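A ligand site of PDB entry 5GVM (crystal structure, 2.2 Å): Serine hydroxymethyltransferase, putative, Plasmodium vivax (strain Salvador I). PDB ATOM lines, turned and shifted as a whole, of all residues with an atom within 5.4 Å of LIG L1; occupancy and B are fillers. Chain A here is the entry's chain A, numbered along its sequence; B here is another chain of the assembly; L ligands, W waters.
Residues that only touch LIG L1: Asn 105, His 129, Tyr 182, Thr 183, Thr 234, Lys 237, Glu 56 of chain B and Gly 271 of chain B. Hydrophobic or aromatic side chains that line LIG L1: His 129, His 211, His 236, Tyr 54 of chain B and Tyr 64 of chain B. 20 residues have an atom within 4 Å of LIG L1: Ser 34, Ser 100, Gly 101, Ser 102, Asn 105, His 129, Tyr 182, Thr 183, Asp 208, Ser 210, His 211, Thr 234, His 236, Lys 237, Arg 371, Tyr 54 of chain B, Glu 56 of chain B, Tyr 64 of chain B, Gly 271 of chain B and Gly 272 of chain B. The nearest printed residue that does not touch LIG L1 is Thr 131 (4.5 Å).
Water W1 lies within hydrogen-bond range of an oxygen (O4) of LIG L1 (2.9 Å), the backbone NH (N) of Gly 271 of chain B (3.1 Å), the backbone carbonyl oxygen (O) of Gly 272 of chain B (3.2 Å) and the side-chain hydroxyl (OG) of Ser 100 (3.5 Å). Water W2 lies within hydrogen-bond range of NH2 of Arg 243 (2.7 Å), O5 of LIG L1 (3.0 Å), O of Gly 272 of chain B (3.0 Å) and OG of Ser 100 (3.3 Å).
A ring nitrogen (NE2) of His 211 is in hydrogen-bond range of an oxygen (O6) of LIG L1, at 2.5 Å. The backbone NH of Gly 272 of chain B is in hydrogen-bond range of an oxygen (O3) of LIG L1, 3.0 Å away. An oxygen (O7) of LIG L1 lies within hydrogen-bond range of the side-chain hydroxyl (OG) of Ser 34 (2.7 Å). The side-chain hydroxyl (OH) of Tyr 64 of chain B lies within hydrogen-bond range of an oxygen (O7) of LIG L1. The side-chain carboxylate (OE1) of Glu 56 of chain B lies close to a nitrogen (N3) of LG2 L2 (3.1 Å). OG of Ser 100 is in hydrogen-bond range of O5 of LIG L1 (2.7 Å). OG of Ser 210 lies within hydrogen-bond range of N1 of LIG L1, at 3.4 Å. The guanidinium group (NH1) of Arg 371 lies within salt-bridge range of an oxygen (O6) of LIG L1 (2.7 Å). O4 of LIG L1 lies within hydrogen-bond range of OG of Ser 102, at 2.6 Å. An oxygen (O3) of LG2 L2 lies within hydrogen-bond range of the side-chain hydroxyl (OG1) of Thr 183 (3.1 Å). O5 of LIG L1 lies within hydrogen-bond range of NE2 of His 236, at 3.1 Å. The side-chain carboxylate (OD2) of Asp 208 is in hydrogen-bond range of a nitrogen (N1) of LIG L1. The backbone NH of Ser 102 sits at hydrogen-bond distance from an oxygen (O4) of LIG L1 (2.9 Å). N of Gly 101 sits at hydrogen-bond distance from O5 of LIG L1. The side-chain hydroxyl of Tyr 54 of chain B is in hydrogen-bond range of an oxygen (O3) of LIG L1 (2.6 Å).
The side-chain hydroxyl of Ser 102 lies within hydrogen-bond range of the backbone NH of Gly 271 of chain B, 3.1 Å away. A ring nitrogen (NE2) of His 274 of chain B lies within hydrogen-bond range of the side-chain hydroxyl (OG) of Ser 100, at 2.9 Å. O of Thr 183 lies within hydrogen-bond range of NE2 of His 211, at 3.3 Å. OG of Ser 210 is in hydrogen-bond range of OD1 of Asp 208, 2.6 Å away. OH of Tyr 54 of chain B is in hydrogen-bond range of NZ of Lys 237 (3.1 Å). The side-chain hydroxyl (OG1) of Thr 131 sits at hydrogen-bond distance from the side-chain amide nitrogen (ND2) of Asn 105 (2.9 Å). OG of Ser 34 sits at hydrogen-bond distance from NH2 of Arg 371. A ring nitrogen (NE2) of His 236 sits at hydrogen-bond distance from the side-chain amino group (NZ) of Lys 237 (3.4 Å).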
ATOM      1  N   ILE A  32     -15.652 -22.186 -11.414  1.00  0.00           N
ATOM      2  CA  ILE A  32     -14.808 -22.170 -10.199  1.00  0.00           C
ATOM      3  C   ILE A  32     -14.603 -20.705  -9.817  1.00  0.00           C
ATOM      4  O   ILE A  32     -14.114 -19.913 -10.616  1.00  0.00           O
ATOM      5  CB  ILE A  32     -13.425 -22.836 -10.374  1.00  0.00           C
ATOM      6  CG1 ILE A  32     -13.545 -24.266 -10.943  1.00  0.00           C
ATOM      7  CG2 ILE A  32     -12.688 -22.859  -9.049  1.00  0.00           C
ATOM      8  CD1 ILE A  32     -13.976 -25.310  -9.946  1.00  0.00           C
ATOM      9  N   SER A  34     -12.688 -19.134  -7.861  1.00  0.00           N
ATOM     10  CA  SER A  34     -11.260 -18.727  -7.820  1.00  0.00           C
ATOM     11  C   SER A  34     -10.490 -18.821  -9.147  1.00  0.00           C
ATOM     12  O   SER A  34      -9.291 -18.626  -9.137  1.00  0.00           O
ATOM     13  CB  SER A  34     -10.553 -19.592  -6.788  1.00  0.00           C
ATOM     14  OG  SER A  34     -10.838 -20.942  -7.033  1.00  0.00           O
ATOM     15  N   SER A 100       2.642 -17.227  -3.773  1.00  0.00           N
ATOM     16  CA  SER A 100       1.205 -17.494  -3.933  1.00  0.00           C
ATOM     17  C   SER A 100       0.475 -17.032  -2.669  1.00  0.00           C
ATOM     18  O   SER A 100       1.115 -16.591  -1.722  1.00  0.00           O
ATOM     19  CB  SER A 100       0.935 -19.006  -4.163  1.00  0.00           C
ATOM     20  OG  SER A 100       0.008 -19.214  -5.246  1.00  0.00           O
ATOM     21  N   GLY A 101      -0.861 -17.158  -2.676  1.00  0.00           N
ATOM     22  CA  GLY A 101      -1.676 -16.653  -1.578  1.00  0.00           C
ATOM     23  C   GLY A 101      -1.407 -17.234  -0.205  1.00  0.00           C
ATOM     24  O   GLY A 101      -1.416 -16.513   0.822  1.00  0.00           O
ATOM     25  N   SER A 102      -1.191 -18.544  -0.175  1.00  0.00           N
ATOM     26  CA  SER A 102      -0.960 -19.234   1.080  1.00  0.00           C
ATOM     27  C   SER A 102       0.379 -18.753   1.664  1.00  0.00           C
ATOM     28  O   SER A 102       0.461 -18.495   2.868  1.00  0.00           O
ATOM     29  CB  SER A 102      -0.988 -20.764   0.922  1.00  0.00           C
ATOM     30  OG  SER A 102      -2.207 -21.236   0.331  1.00  0.00           O
ATOM     31  N   ALA A 103       1.395 -18.627   0.812  1.00  0.00           N
ATOM     32  CA  ALA A 103       2.699 -18.143   1.261  1.00  0.00           C
ATOM     33  C   ALA A 103       2.629 -16.712   1.845  1.00  0.00           C
ATOM     34  O   ALA A 103       3.047 -16.490   2.969  1.00  0.00           O
ATOM     35  CB  ALA A 103       3.747 -18.261   0.163  1.00  0.00           C
ATOM     36  N   ASN A 105       0.094 -15.174   3.121  1.00  0.00           N
ATOM     37  CA  ASN A 105      -0.612 -15.169   4.392  1.00  0.00           C
ATOM     38  C   ASN A 105       0.264 -15.649   5.548  1.00  0.00           C
ATOM     39  O   ASN A 105       0.324 -14.972   6.578  1.00  0.00           O
ATOM     40  CB  ASN A 105      -1.913 -15.995   4.349  1.00  0.00           C
ATOM     41  CG  ASN A 105      -3.019 -15.312   3.559  1.00  0.00           C
ATOM     42  OD1 ASN A 105      -2.885 -14.184   3.127  1.00  0.00           O
ATOM     43  ND2 ASN A 105      -4.140 -16.002   3.404  1.00  0.00           N
ATOM     44  N   HIS A 129     -10.476 -19.425   4.788  1.00  0.00           N
ATOM     45  CA  HIS A 129      -9.383 -20.162   4.164  1.00  0.00           C
ATOM     46  C   HIS A 129      -8.609 -21.076   5.122  1.00  0.00           C
ATOM     47  O   HIS A 129      -8.610 -20.873   6.322  1.00  0.00           O
ATOM     48  CB  HIS A 129      -8.405 -19.223   3.446  1.00  0.00           C
ATOM     49  CG  HIS A 129      -7.544 -19.931   2.433  1.00  0.00           C
ATOM     50  ND1 HIS A 129      -6.181 -19.992   2.537  1.00  0.00           N
ATOM     51  CD2 HIS A 129      -7.878 -20.684   1.361  1.00  0.00           C
ATOM     52  CE1 HIS A 129      -5.690 -20.721   1.549  1.00  0.00           C
ATOM     53  NE2 HIS A 129      -6.712 -21.154   0.824  1.00  0.00           N
ATOM     54  N   THR A 131      -5.417 -21.135   5.408  1.00  0.00           N
ATOM     55  CA  THR A 131      -4.384 -20.255   6.019  1.00  0.00           C
ATOM     56  C   THR A 131      -4.903 -19.228   7.030  1.00  0.00           C
ATOM     57  O   THR A 131      -4.157 -18.358   7.461  1.00  0.00           O
ATOM     58  CB  THR A 131      -3.566 -19.515   4.929  1.00  0.00           C
ATOM     59  OG1 THR A 131      -4.432 -18.770   4.071  1.00  0.00           O
ATOM     60  CG2 THR A 131      -2.769 -20.528   4.113  1.00  0.00           C
ATOM     61  N   HIS A 132      -6.163 -19.336   7.461  1.00  0.00           N
ATOM     62  CA  HIS A 132      -6.697 -18.481   8.518  1.00  0.00           C
ATOM     63  C   HIS A 132      -6.724 -19.192   9.872  1.00  0.00           C
ATOM     64  O   HIS A 132      -7.459 -18.796  10.774  1.00  0.00           O
ATOM     65  CB  HIS A 132      -8.074 -17.914   8.106  1.00  0.00           C
ATOM     66  CG  HIS A 132      -8.032 -17.128   6.833  1.00  0.00           C
ATOM     67  ND1 HIS A 132      -9.173 -16.733   6.165  1.00  0.00           N
ATOM     68  CD2 HIS A 132      -7.001 -16.664   6.095  1.00  0.00           C
ATOM     69  CE1 HIS A 132      -8.838 -16.049   5.088  1.00  0.00           C
ATOM     70  NE2 HIS A 132      -7.527 -16.006   5.007  1.00  0.00           N
ATOM     71  N   GLY A 181     -12.132 -11.546   5.503  1.00  0.00           N
ATOM     72  CA  GLY A 181     -11.972 -11.779   4.029  1.00  0.00           C
ATOM     73  C   GLY A 181     -11.691 -13.264   3.802  1.00  0.00           C
ATOM     74  O   GLY A 181     -10.856 -13.847   4.481  1.00  0.00           O
ATOM     75  N   TYR A 182     -12.416 -13.879   2.861  1.00  0.00           N
ATOM     76  CA  TYR A 182     -12.713 -15.315   2.951  1.00  0.00           C
ATOM     77  C   TYR A 182     -12.664 -16.006   1.597  1.00  0.00           C
ATOM     78  O   TYR A 182     -12.418 -15.352   0.585  1.00  0.00           O
ATOM     79  CB  TYR A 182     -14.087 -15.475   3.594  1.00  0.00           C
ATOM     80  CG  TYR A 182     -14.305 -14.696   4.878  1.00  0.00           C
ATOM     81  CD1 TYR A 182     -13.543 -14.974   6.024  1.00  0.00           C
ATOM     82  CD2 TYR A 182     -15.278 -13.690   4.966  1.00  0.00           C
ATOM     83  CE1 TYR A 182     -13.737 -14.275   7.211  1.00  0.00           C
ATOM     84  CE2 TYR A 182     -15.482 -12.990   6.154  1.00  0.00           C
ATOM     85  CZ  TYR A 182     -14.712 -13.293   7.281  1.00  0.00           C
ATOM     86  OH  TYR A 182     -14.886 -12.594   8.468  1.00  0.00           O
ATOM     87  N   THR A 183     -12.891 -17.311   1.572  1.00  0.00           N
ATOM     88  CA  THR A 183     -12.813 -18.085   0.293  1.00  0.00           C
ATOM     89  C   THR A 183     -14.177 -18.429  -0.288  1.00  0.00           C
ATOM     90  O   THR A 183     -14.357 -18.336  -1.503  1.00  0.00           O
ATOM     91  CB  THR A 183     -11.913 -19.349   0.338  1.00  0.00           C
ATOM     92  OG1 THR A 183     -12.671 -20.562   0.200  1.00  0.00           O
ATOM     93  CG2 THR A 183     -11.131 -19.407   1.573  1.00  0.00           C
ATOM     94  N   ASP A 208      -7.883 -10.429   3.962  1.00  0.00           N
ATOM     95  CA  ASP A 208      -7.400 -11.236   2.829  1.00  0.00           C
ATOM     96  C   ASP A 208      -8.482 -11.085   1.829  1.00  0.00           C
ATOM     97  O   ASP A 208      -9.535 -11.646   2.031  1.00  0.00           O
ATOM     98  CB  ASP A 208      -7.227 -12.710   3.198  1.00  0.00           C
ATOM     99  CG  ASP A 208      -6.779 -13.582   2.005  1.00  0.00           C
ATOM    100  OD1 ASP A 208      -6.979 -13.220   0.817  1.00  0.00           O
ATOM    101  OD2 ASP A 208      -6.217 -14.656   2.258  1.00  0.00           O
ATOM    102  N   SER A 210      -8.296 -11.816  -1.555  1.00  0.00           N
ATOM    103  CA  SER A 210      -7.996 -12.640  -2.736  1.00  0.00           C
ATOM    104  C   SER A 210      -9.218 -12.852  -3.657  1.00  0.00           C
ATOM    105  O   SER A 210      -9.151 -12.598  -4.854  1.00  0.00           O
ATOM    106  CB  SER A 210      -7.427 -13.993  -2.293  1.00  0.00           C
ATOM    107  OG  SER A 210      -6.175 -13.831  -1.609  1.00  0.00           O
ATOM    108  N   HIS A 211     -10.342 -13.262  -3.066  1.00  0.00           N
ATOM    109  CA  HIS A 211     -11.598 -13.476  -3.814  1.00  0.00           C
ATOM    110  C   HIS A 211     -12.384 -12.270  -4.278  1.00  0.00           C
ATOM    111  O   HIS A 211     -13.221 -12.409  -5.160  1.00  0.00           O
ATOM    112  CB  HIS A 211     -12.533 -14.387  -3.038  1.00  0.00           C
ATOM    113  CG  HIS A 211     -12.334 -15.828  -3.368  1.00  0.00           C
ATOM    114  ND1 HIS A 211     -12.914 -16.412  -4.461  1.00  0.00           N
ATOM    115  CD2 HIS A 211     -11.575 -16.773  -2.784  1.00  0.00           C
ATOM    116  CE1 HIS A 211     -12.539 -17.676  -4.524  1.00  0.00           C
ATOM    117  NE2 HIS A 211     -11.730 -17.918  -3.514  1.00  0.00           N
ATOM    118  N   THR A 234      -4.174 -12.647  -3.640  1.00  0.00           N
ATOM    119  CA  THR A 234      -3.628 -13.351  -4.784  1.00  0.00           C
ATOM    120  C   THR A 234      -3.933 -12.524  -5.998  1.00  0.00           C
ATOM    121  O   THR A 234      -4.835 -11.714  -5.971  1.00  0.00           O
ATOM    122  CB  THR A 234      -4.293 -14.717  -4.975  1.00  0.00           C
ATOM    123  OG1 THR A 234      -5.713 -14.554  -5.077  1.00  0.00           O
ATOM    124  CG2 THR A 234      -3.983 -15.618  -3.829  1.00  0.00           C
ATOM    125  N   HIS A 236      -4.412 -14.111  -9.204  1.00  0.00           N
ATOM    126  CA  HIS A 236      -4.883 -15.089 -10.231  1.00  0.00           C
ATOM    127  C   HIS A 236      -6.396 -15.362 -10.295  1.00  0.00           C
ATOM    128  O   HIS A 236      -6.864 -16.086 -11.195  1.00  0.00           O
ATOM    129  CB  HIS A 236      -4.175 -16.452 -10.121  1.00  0.00           C
ATOM    130  CG  HIS A 236      -4.043 -16.982  -8.721  1.00  0.00           C
ATOM    131  ND1 HIS A 236      -3.066 -16.528  -7.853  1.00  0.00           N
ATOM    132  CD2 HIS A 236      -4.714 -17.947  -8.062  1.00  0.00           C
ATOM    133  CE1 HIS A 236      -3.149 -17.205  -6.723  1.00  0.00           C
ATOM    134  NE2 HIS A 236      -4.143 -18.062  -6.817  1.00  0.00           N
ATOM    135  N   LYS A 237      -7.145 -14.816  -9.343  1.00  0.00           N
ATOM    136  CA  LYS A 237      -8.572 -15.005  -9.308  1.00  0.00           C
ATOM    137  C   LYS A 237      -9.291 -13.869 -10.100  1.00  0.00           C
ATOM    138  O   LYS A 237      -9.025 -13.648 -11.286  1.00  0.00           O
ATOM    139  CB  LYS A 237      -9.046 -15.145  -7.860  1.00  0.00           C
ATOM    140  CG  LYS A 237      -8.302 -16.194  -7.053  1.00  0.00           C
ATOM    141  CD  LYS A 237      -8.886 -16.261  -5.661  1.00  0.00           C
ATOM    142  CE  LYS A 237      -8.274 -17.373  -4.826  1.00  0.00           C
ATOM    143  NZ  LYS A 237      -6.801 -17.352  -4.824  1.00  0.00           N
ATOM    144  N   ARG A 243      -0.435 -16.508 -11.323  1.00  0.00           N
ATOM    145  CA  ARG A 243      -0.478 -17.098  -9.978  1.00  0.00           C
ATOM    146  C   ARG A 243       0.607 -16.439  -9.108  1.00  0.00           C
ATOM    147  O   ARG A 243       1.764 -16.741  -9.233  1.00  0.00           O
ATOM    148  CB  ARG A 243      -0.331 -18.630 -10.014  1.00  0.00           C
ATOM    149  CG  ARG A 243      -1.310 -19.324 -10.961  1.00  0.00           C
ATOM    150  CD  ARG A 243      -1.277 -20.852 -10.793  1.00  0.00           C
ATOM    151  NE  ARG A 243      -2.113 -21.287  -9.674  1.00  0.00           N
ATOM    152  CZ  ARG A 243      -3.436 -21.328  -9.679  1.00  0.00           C
ATOM    153  NH1 ARG A 243      -4.132 -20.962 -10.747  1.00  0.00           N
ATOM    154  NH2 ARG A 243      -4.082 -21.730  -8.587  1.00  0.00           N
ATOM    155  N   ASN A 354     -16.759 -26.546  -7.597  1.00  0.00           N
ATOM    156  CA  ASN A 354     -16.265 -27.313  -6.477  1.00  0.00           C
ATOM    157  C   ASN A 354     -17.308 -27.588  -5.423  1.00  0.00           C
ATOM    158  O   ASN A 354     -18.234 -26.787  -5.215  1.00  0.00           O
ATOM    159  CB  ASN A 354     -14.999 -26.675  -5.862  1.00  0.00           C
ATOM    160  CG  ASN A 354     -15.271 -25.350  -5.205  1.00  0.00           C
ATOM    161  OD1 ASN A 354     -15.157 -24.308  -5.838  1.00  0.00           O
ATOM    162  ND2 ASN A 354     -15.637 -25.377  -3.935  1.00  0.00           N
ATOM    163  N   ARG A 371     -19.941 -24.511  -4.457  1.00  0.00           N
ATOM    164  CA  ARG A 371     -19.682 -23.134  -4.716  1.00  0.00           C
ATOM    165  C   ARG A 371     -19.530 -22.950  -6.228  1.00  0.00           C
ATOM    166  O   ARG A 371     -18.901 -23.781  -6.906  1.00  0.00           O
ATOM    167  CB  ARG A 371     -18.429 -22.685  -3.980  1.00  0.00           C
ATOM    168  CG  ARG A 371     -18.008 -21.239  -4.227  1.00  0.00           C
ATOM    169  CD  ARG A 371     -16.637 -20.969  -3.663  1.00  0.00           C
ATOM    170  NE  ARG A 371     -15.585 -21.569  -4.484  1.00  0.00           N
ATOM    171  CZ  ARG A 371     -14.272 -21.360  -4.353  1.00  0.00           C
ATOM    172  NH1 ARG A 371     -13.799 -20.542  -3.396  1.00  0.00           N
ATOM    173  NH2 ARG A 371     -13.442 -21.977  -5.185  1.00  0.00           N
ATOM    174  N   TYR B  54      -7.024 -24.377 -11.026  1.00  0.00           N
ATOM    175  CA  TYR B  54      -6.904 -24.688  -9.599  1.00  0.00           C
ATOM    176  C   TYR B  54      -6.999 -26.210  -9.413  1.00  0.00           C
ATOM    177  O   TYR B  54      -7.902 -26.860  -9.940  1.00  0.00           O
ATOM    178  CB  TYR B  54      -8.002 -24.012  -8.758  1.00  0.00           C
ATOM    179  CG  TYR B  54      -7.442 -23.003  -7.796  1.00  0.00           C
ATOM    180  CD1 TYR B  54      -6.707 -23.422  -6.694  1.00  0.00           C
ATOM    181  CD2 TYR B  54      -7.633 -21.646  -7.991  1.00  0.00           C
ATOM    182  CE1 TYR B  54      -6.173 -22.508  -5.803  1.00  0.00           C
ATOM    183  CE2 TYR B  54      -7.099 -20.720  -7.116  1.00  0.00           C
ATOM    184  CZ  TYR B  54      -6.365 -21.164  -6.031  1.00  0.00           C
ATOM    185  OH  TYR B  54      -5.823 -20.250  -5.191  1.00  0.00           O
ATOM    186  N   GLU B  56      -5.906 -28.030  -6.164  1.00  0.00           N
ATOM    187  CA  GLU B  56      -5.437 -28.311  -4.805  1.00  0.00           C
ATOM    188  C   GLU B  56      -5.625 -29.777  -4.451  1.00  0.00           C
ATOM    189  O   GLU B  56      -6.666 -30.340  -4.750  1.00  0.00           O
ATOM    190  CB  GLU B  56      -6.151 -27.472  -3.746  1.00  0.00           C
ATOM    191  CG  GLU B  56      -6.058 -25.973  -3.987  1.00  0.00           C
ATOM    192  CD  GLU B  56      -6.508 -25.126  -2.825  1.00  0.00           C
ATOM    193  OE1 GLU B  56      -6.851 -25.681  -1.787  1.00  0.00           O
ATOM    194  OE2 GLU B  56      -6.490 -23.887  -2.947  1.00  0.00           O
ATOM    195  N   TYR B  64     -11.327 -29.648  -6.985  1.00  0.00           N
ATOM    196  CA  TYR B  64     -12.023 -28.958  -8.085  1.00  0.00           C
ATOM    197  C   TYR B  64     -12.327 -29.896  -9.246  1.00  0.00           C
ATOM    198  O   TYR B  64     -11.640 -30.909  -9.486  1.00  0.00           O
ATOM    199  CB  TYR B  64     -11.227 -27.717  -8.589  1.00  0.00           C
ATOM    200  CG  TYR B  64     -10.866 -26.813  -7.454  1.00  0.00           C
ATOM    201  CD1 TYR B  64      -9.706 -27.027  -6.726  1.00  0.00           C
ATOM    202  CD2 TYR B  64     -11.707 -25.773  -7.054  1.00  0.00           C
ATOM    203  CE1 TYR B  64      -9.370 -26.224  -5.654  1.00  0.00           C
ATOM    204  CE2 TYR B  64     -11.390 -24.967  -5.968  1.00  0.00           C
ATOM    205  CZ  TYR B  64     -10.222 -25.194  -5.274  1.00  0.00           C
ATOM    206  OH  TYR B  64      -9.857 -24.408  -4.215  1.00  0.00           O
ATOM    207  N   GLN B 270       1.105 -24.980   1.358  1.00  0.00           N
ATOM    208  CA  GLN B 270       0.677 -24.445   0.075  1.00  0.00           C
ATOM    209  C   GLN B 270      -0.835 -24.562  -0.097  1.00  0.00           C
ATOM    210  O   GLN B 270      -1.492 -25.238   0.677  1.00  0.00           O
ATOM    211  CB  GLN B 270       1.444 -25.115  -1.082  1.00  0.00           C
ATOM    212  CG  GLN B 270       2.963 -25.126  -0.856  1.00  0.00           C
ATOM    213  CD  GLN B 270       3.809 -25.136  -2.133  1.00  0.00           C
ATOM    214  OE1 GLN B 270       4.938 -24.587  -2.157  1.00  0.00           O
ATOM    215  NE2 GLN B 270       3.310 -25.771  -3.165  1.00  0.00           N
ATOM    216  N   GLY B 271      -1.356 -23.845  -1.080  1.00  0.00           N
ATOM    217  CA  GLY B 271      -2.693 -24.049  -1.618  1.00  0.00           C
ATOM    218  C   GLY B 271      -2.573 -24.648  -3.017  1.00  0.00           C
ATOM    219  O   GLY B 271      -1.986 -25.713  -3.195  1.00  0.00           O
ATOM    220  N   GLY B 272      -3.075 -23.934  -4.014  1.00  0.00           N
ATOM    221  CA  GLY B 272      -3.050 -24.400  -5.400  1.00  0.00           C
ATOM    222  C   GLY B 272      -1.666 -24.611  -5.983  1.00  0.00           C
ATOM    223  O   GLY B 272      -0.820 -23.731  -5.858  1.00  0.00           O
ATOM    224  N   HIS B 274       1.132 -24.806  -9.028  1.00  0.00           N
ATOM    225  CA  HIS B 274       1.349 -23.989 -10.205  1.00  0.00           C
ATOM    226  C   HIS B 274       1.647 -24.946 -11.324  1.00  0.00           C
ATOM    227  O   HIS B 274       2.786 -25.424 -11.480  1.00  0.00           O
ATOM    228  CB  HIS B 274       2.484 -22.999  -9.950  1.00  0.00           C
ATOM    229  CG  HIS B 274       2.115 -21.894  -9.007  1.00  0.00           C
ATOM    230  ND1 HIS B 274       2.859 -20.743  -8.903  1.00  0.00           N
ATOM    231  CD2 HIS B 274       1.089 -21.753  -8.143  1.00  0.00           C
ATOM    232  CE1 HIS B 274       2.308 -19.939  -8.009  1.00  0.00           C
ATOM    233  NE2 HIS B 274       1.234 -20.530  -7.516  1.00  0.00           N
HETATM  234  N1  LIG L   1      -6.754 -16.500   0.471  1.00  0.00           N
HETATM  235  C1  LIG L   1      -8.018 -16.786   0.120  1.00  0.00           C
HETATM  236  C2  LIG L   1      -9.194 -15.972   0.615  1.00  0.00           C
HETATM  237  C3  LIG L   1      -8.220 -17.947  -0.785  1.00  0.00           C
HETATM  238  O1  LIG L   1      -9.456 -18.246  -1.171  1.00  0.00           O
HETATM  239  C4  LIG L   1      -7.063 -18.736  -1.261  1.00  0.00           C
HETATM  240  C5  LIG L   1      -7.197 -19.912  -2.202  1.00  0.00           C
HETATM  241  C6  LIG L   1      -5.730 -18.301  -0.799  1.00  0.00           C
HETATM  242  C7  LIG L   1      -5.671 -17.205   0.071  1.00  0.00           C
HETATM  243  C8  LIG L   1      -4.479 -19.053  -1.199  1.00  0.00           C
HETATM  244  O2  LIG L   1      -4.081 -18.906  -2.566  1.00  0.00           O
HETATM  245  P1  LIG L   1      -3.081 -19.976  -3.239  1.00  0.00           P
HETATM  246  O3  LIG L   1      -4.014 -21.101  -3.597  1.00  0.00           O
HETATM  247  O4  LIG L   1      -2.096 -20.394  -2.175  1.00  0.00           O
HETATM  248  O5  LIG L   1      -2.554 -19.188  -4.403  1.00  0.00           O
HETATM  249  C9  LIG L   1     -10.370 -21.313  -3.631  1.00  0.00           C
HETATM  250  O6  LIG L   1     -11.150 -20.387  -3.368  1.00  0.00           O
HETATM  251  O7  LIG L   1     -10.570 -22.086  -4.570  1.00  0.00           O
HETATM  252  C10 LIG L   1      -9.122 -21.432  -2.771  1.00  0.00           C
HETATM  253  N2  LIG L   1      -8.551 -20.109  -2.648  1.00  0.00           N
HETATM  254  O1  LG2 L   2     -11.132 -33.114   6.968  1.00  0.00           O
HETATM  255  C1  LG2 L   2     -10.527 -32.585   6.010  1.00  0.00           C
HETATM  256  O2  LG2 L   2     -10.456 -33.136   4.885  1.00  0.00           O
HETATM  257  C2  LG2 L   2      -9.871 -31.228   6.231  1.00  0.00           C
HETATM  258  C3  LG2 L   2      -9.624 -30.535   4.899  1.00  0.00           C
HETATM  259  C4  LG2 L   2     -10.699 -29.929   4.226  1.00  0.00           C
HETATM  260  C5  LG2 L   2      -8.350 -30.506   4.372  1.00  0.00           C
HETATM  261  C6  LG2 L   2      -8.143 -29.897   3.139  1.00  0.00           C
HETATM  262  C7  LG2 L   2      -9.207 -29.285   2.458  1.00  0.00           C
HETATM  263  C8  LG2 L   2     -10.479 -29.282   3.009  1.00  0.00           C
HETATM  264  C9  LG2 L   2     -11.586 -28.653   2.242  1.00  0.00           C
HETATM  265  C10 LG2 L   2     -12.722 -29.417   2.018  1.00  0.00           C
HETATM  266  C11 LG2 L   2     -13.773 -28.910   1.259  1.00  0.00           C
HETATM  267  C12 LG2 L   2     -15.001 -29.745   1.021  1.00  0.00           C
HETATM  268  F1  LG2 L   2     -15.954 -29.139   0.372  1.00  0.00           F
HETATM  269  F2  LG2 L   2     -14.621 -30.840   0.398  1.00  0.00           F
HETATM  270  F3  LG2 L   2     -15.562 -30.036   2.158  1.00  0.00           F
HETATM  271  C13 LG2 L   2     -13.678 -27.634   0.714  1.00  0.00           C
HETATM  272  C14 LG2 L   2     -11.491 -27.369   1.703  1.00  0.00           C
HETATM  273  C15 LG2 L   2     -12.542 -26.838   0.911  1.00  0.00           C
HETATM  274  C16 LG2 L   2     -12.522 -25.411   0.355  1.00  0.00           C
HETATM  275  C17 LG2 L   2     -13.136 -25.205  -1.058  1.00  0.00           C
HETATM  276  C18 LG2 L   2     -13.005 -23.762  -1.578  1.00  0.00           C
HETATM  277  C19 LG2 L   2     -12.648 -26.184  -2.146  1.00  0.00           C
HETATM  278  C20 LG2 L   2     -13.371 -24.625   1.363  1.00  0.00           C
HETATM  279  C21 LG2 L   2     -14.536 -25.017   1.631  1.00  0.00           C
HETATM  280  N1  LG2 L   2     -15.602 -25.396   1.857  1.00  0.00           N
HETATM  281  C22 LG2 L   2     -12.949 -23.508   2.008  1.00  0.00           C
HETATM  282  N2  LG2 L   2     -13.685 -22.830   2.884  1.00  0.00           N
HETATM  283  C23 LG2 L   2     -11.132 -24.891   0.381  1.00  0.00           C
HETATM  284  C24 LG2 L   2      -9.836 -25.359  -0.169  1.00  0.00           C
HETATM  285  C25 LG2 L   2      -9.557 -26.569  -1.014  1.00  0.00           C
HETATM  286  N3  LG2 L   2      -8.919 -24.461   0.244  1.00  0.00           N
HETATM  287  N4  LG2 L   2      -9.436 -23.441   1.062  1.00  0.00           N
HETATM  288  C26 LG2 L   2     -10.724 -23.708   1.124  1.00  0.00           C
HETATM  289  O3  LG2 L   2     -11.637 -22.977   1.792  1.00  0.00           O
HETATM  290  O   HOH W   1       0.022 -22.034  -3.247  1.00  0.00           O
HETATM  291  O   HOH W   2      -2.330 -21.207  -6.553  1.00  0.00           O
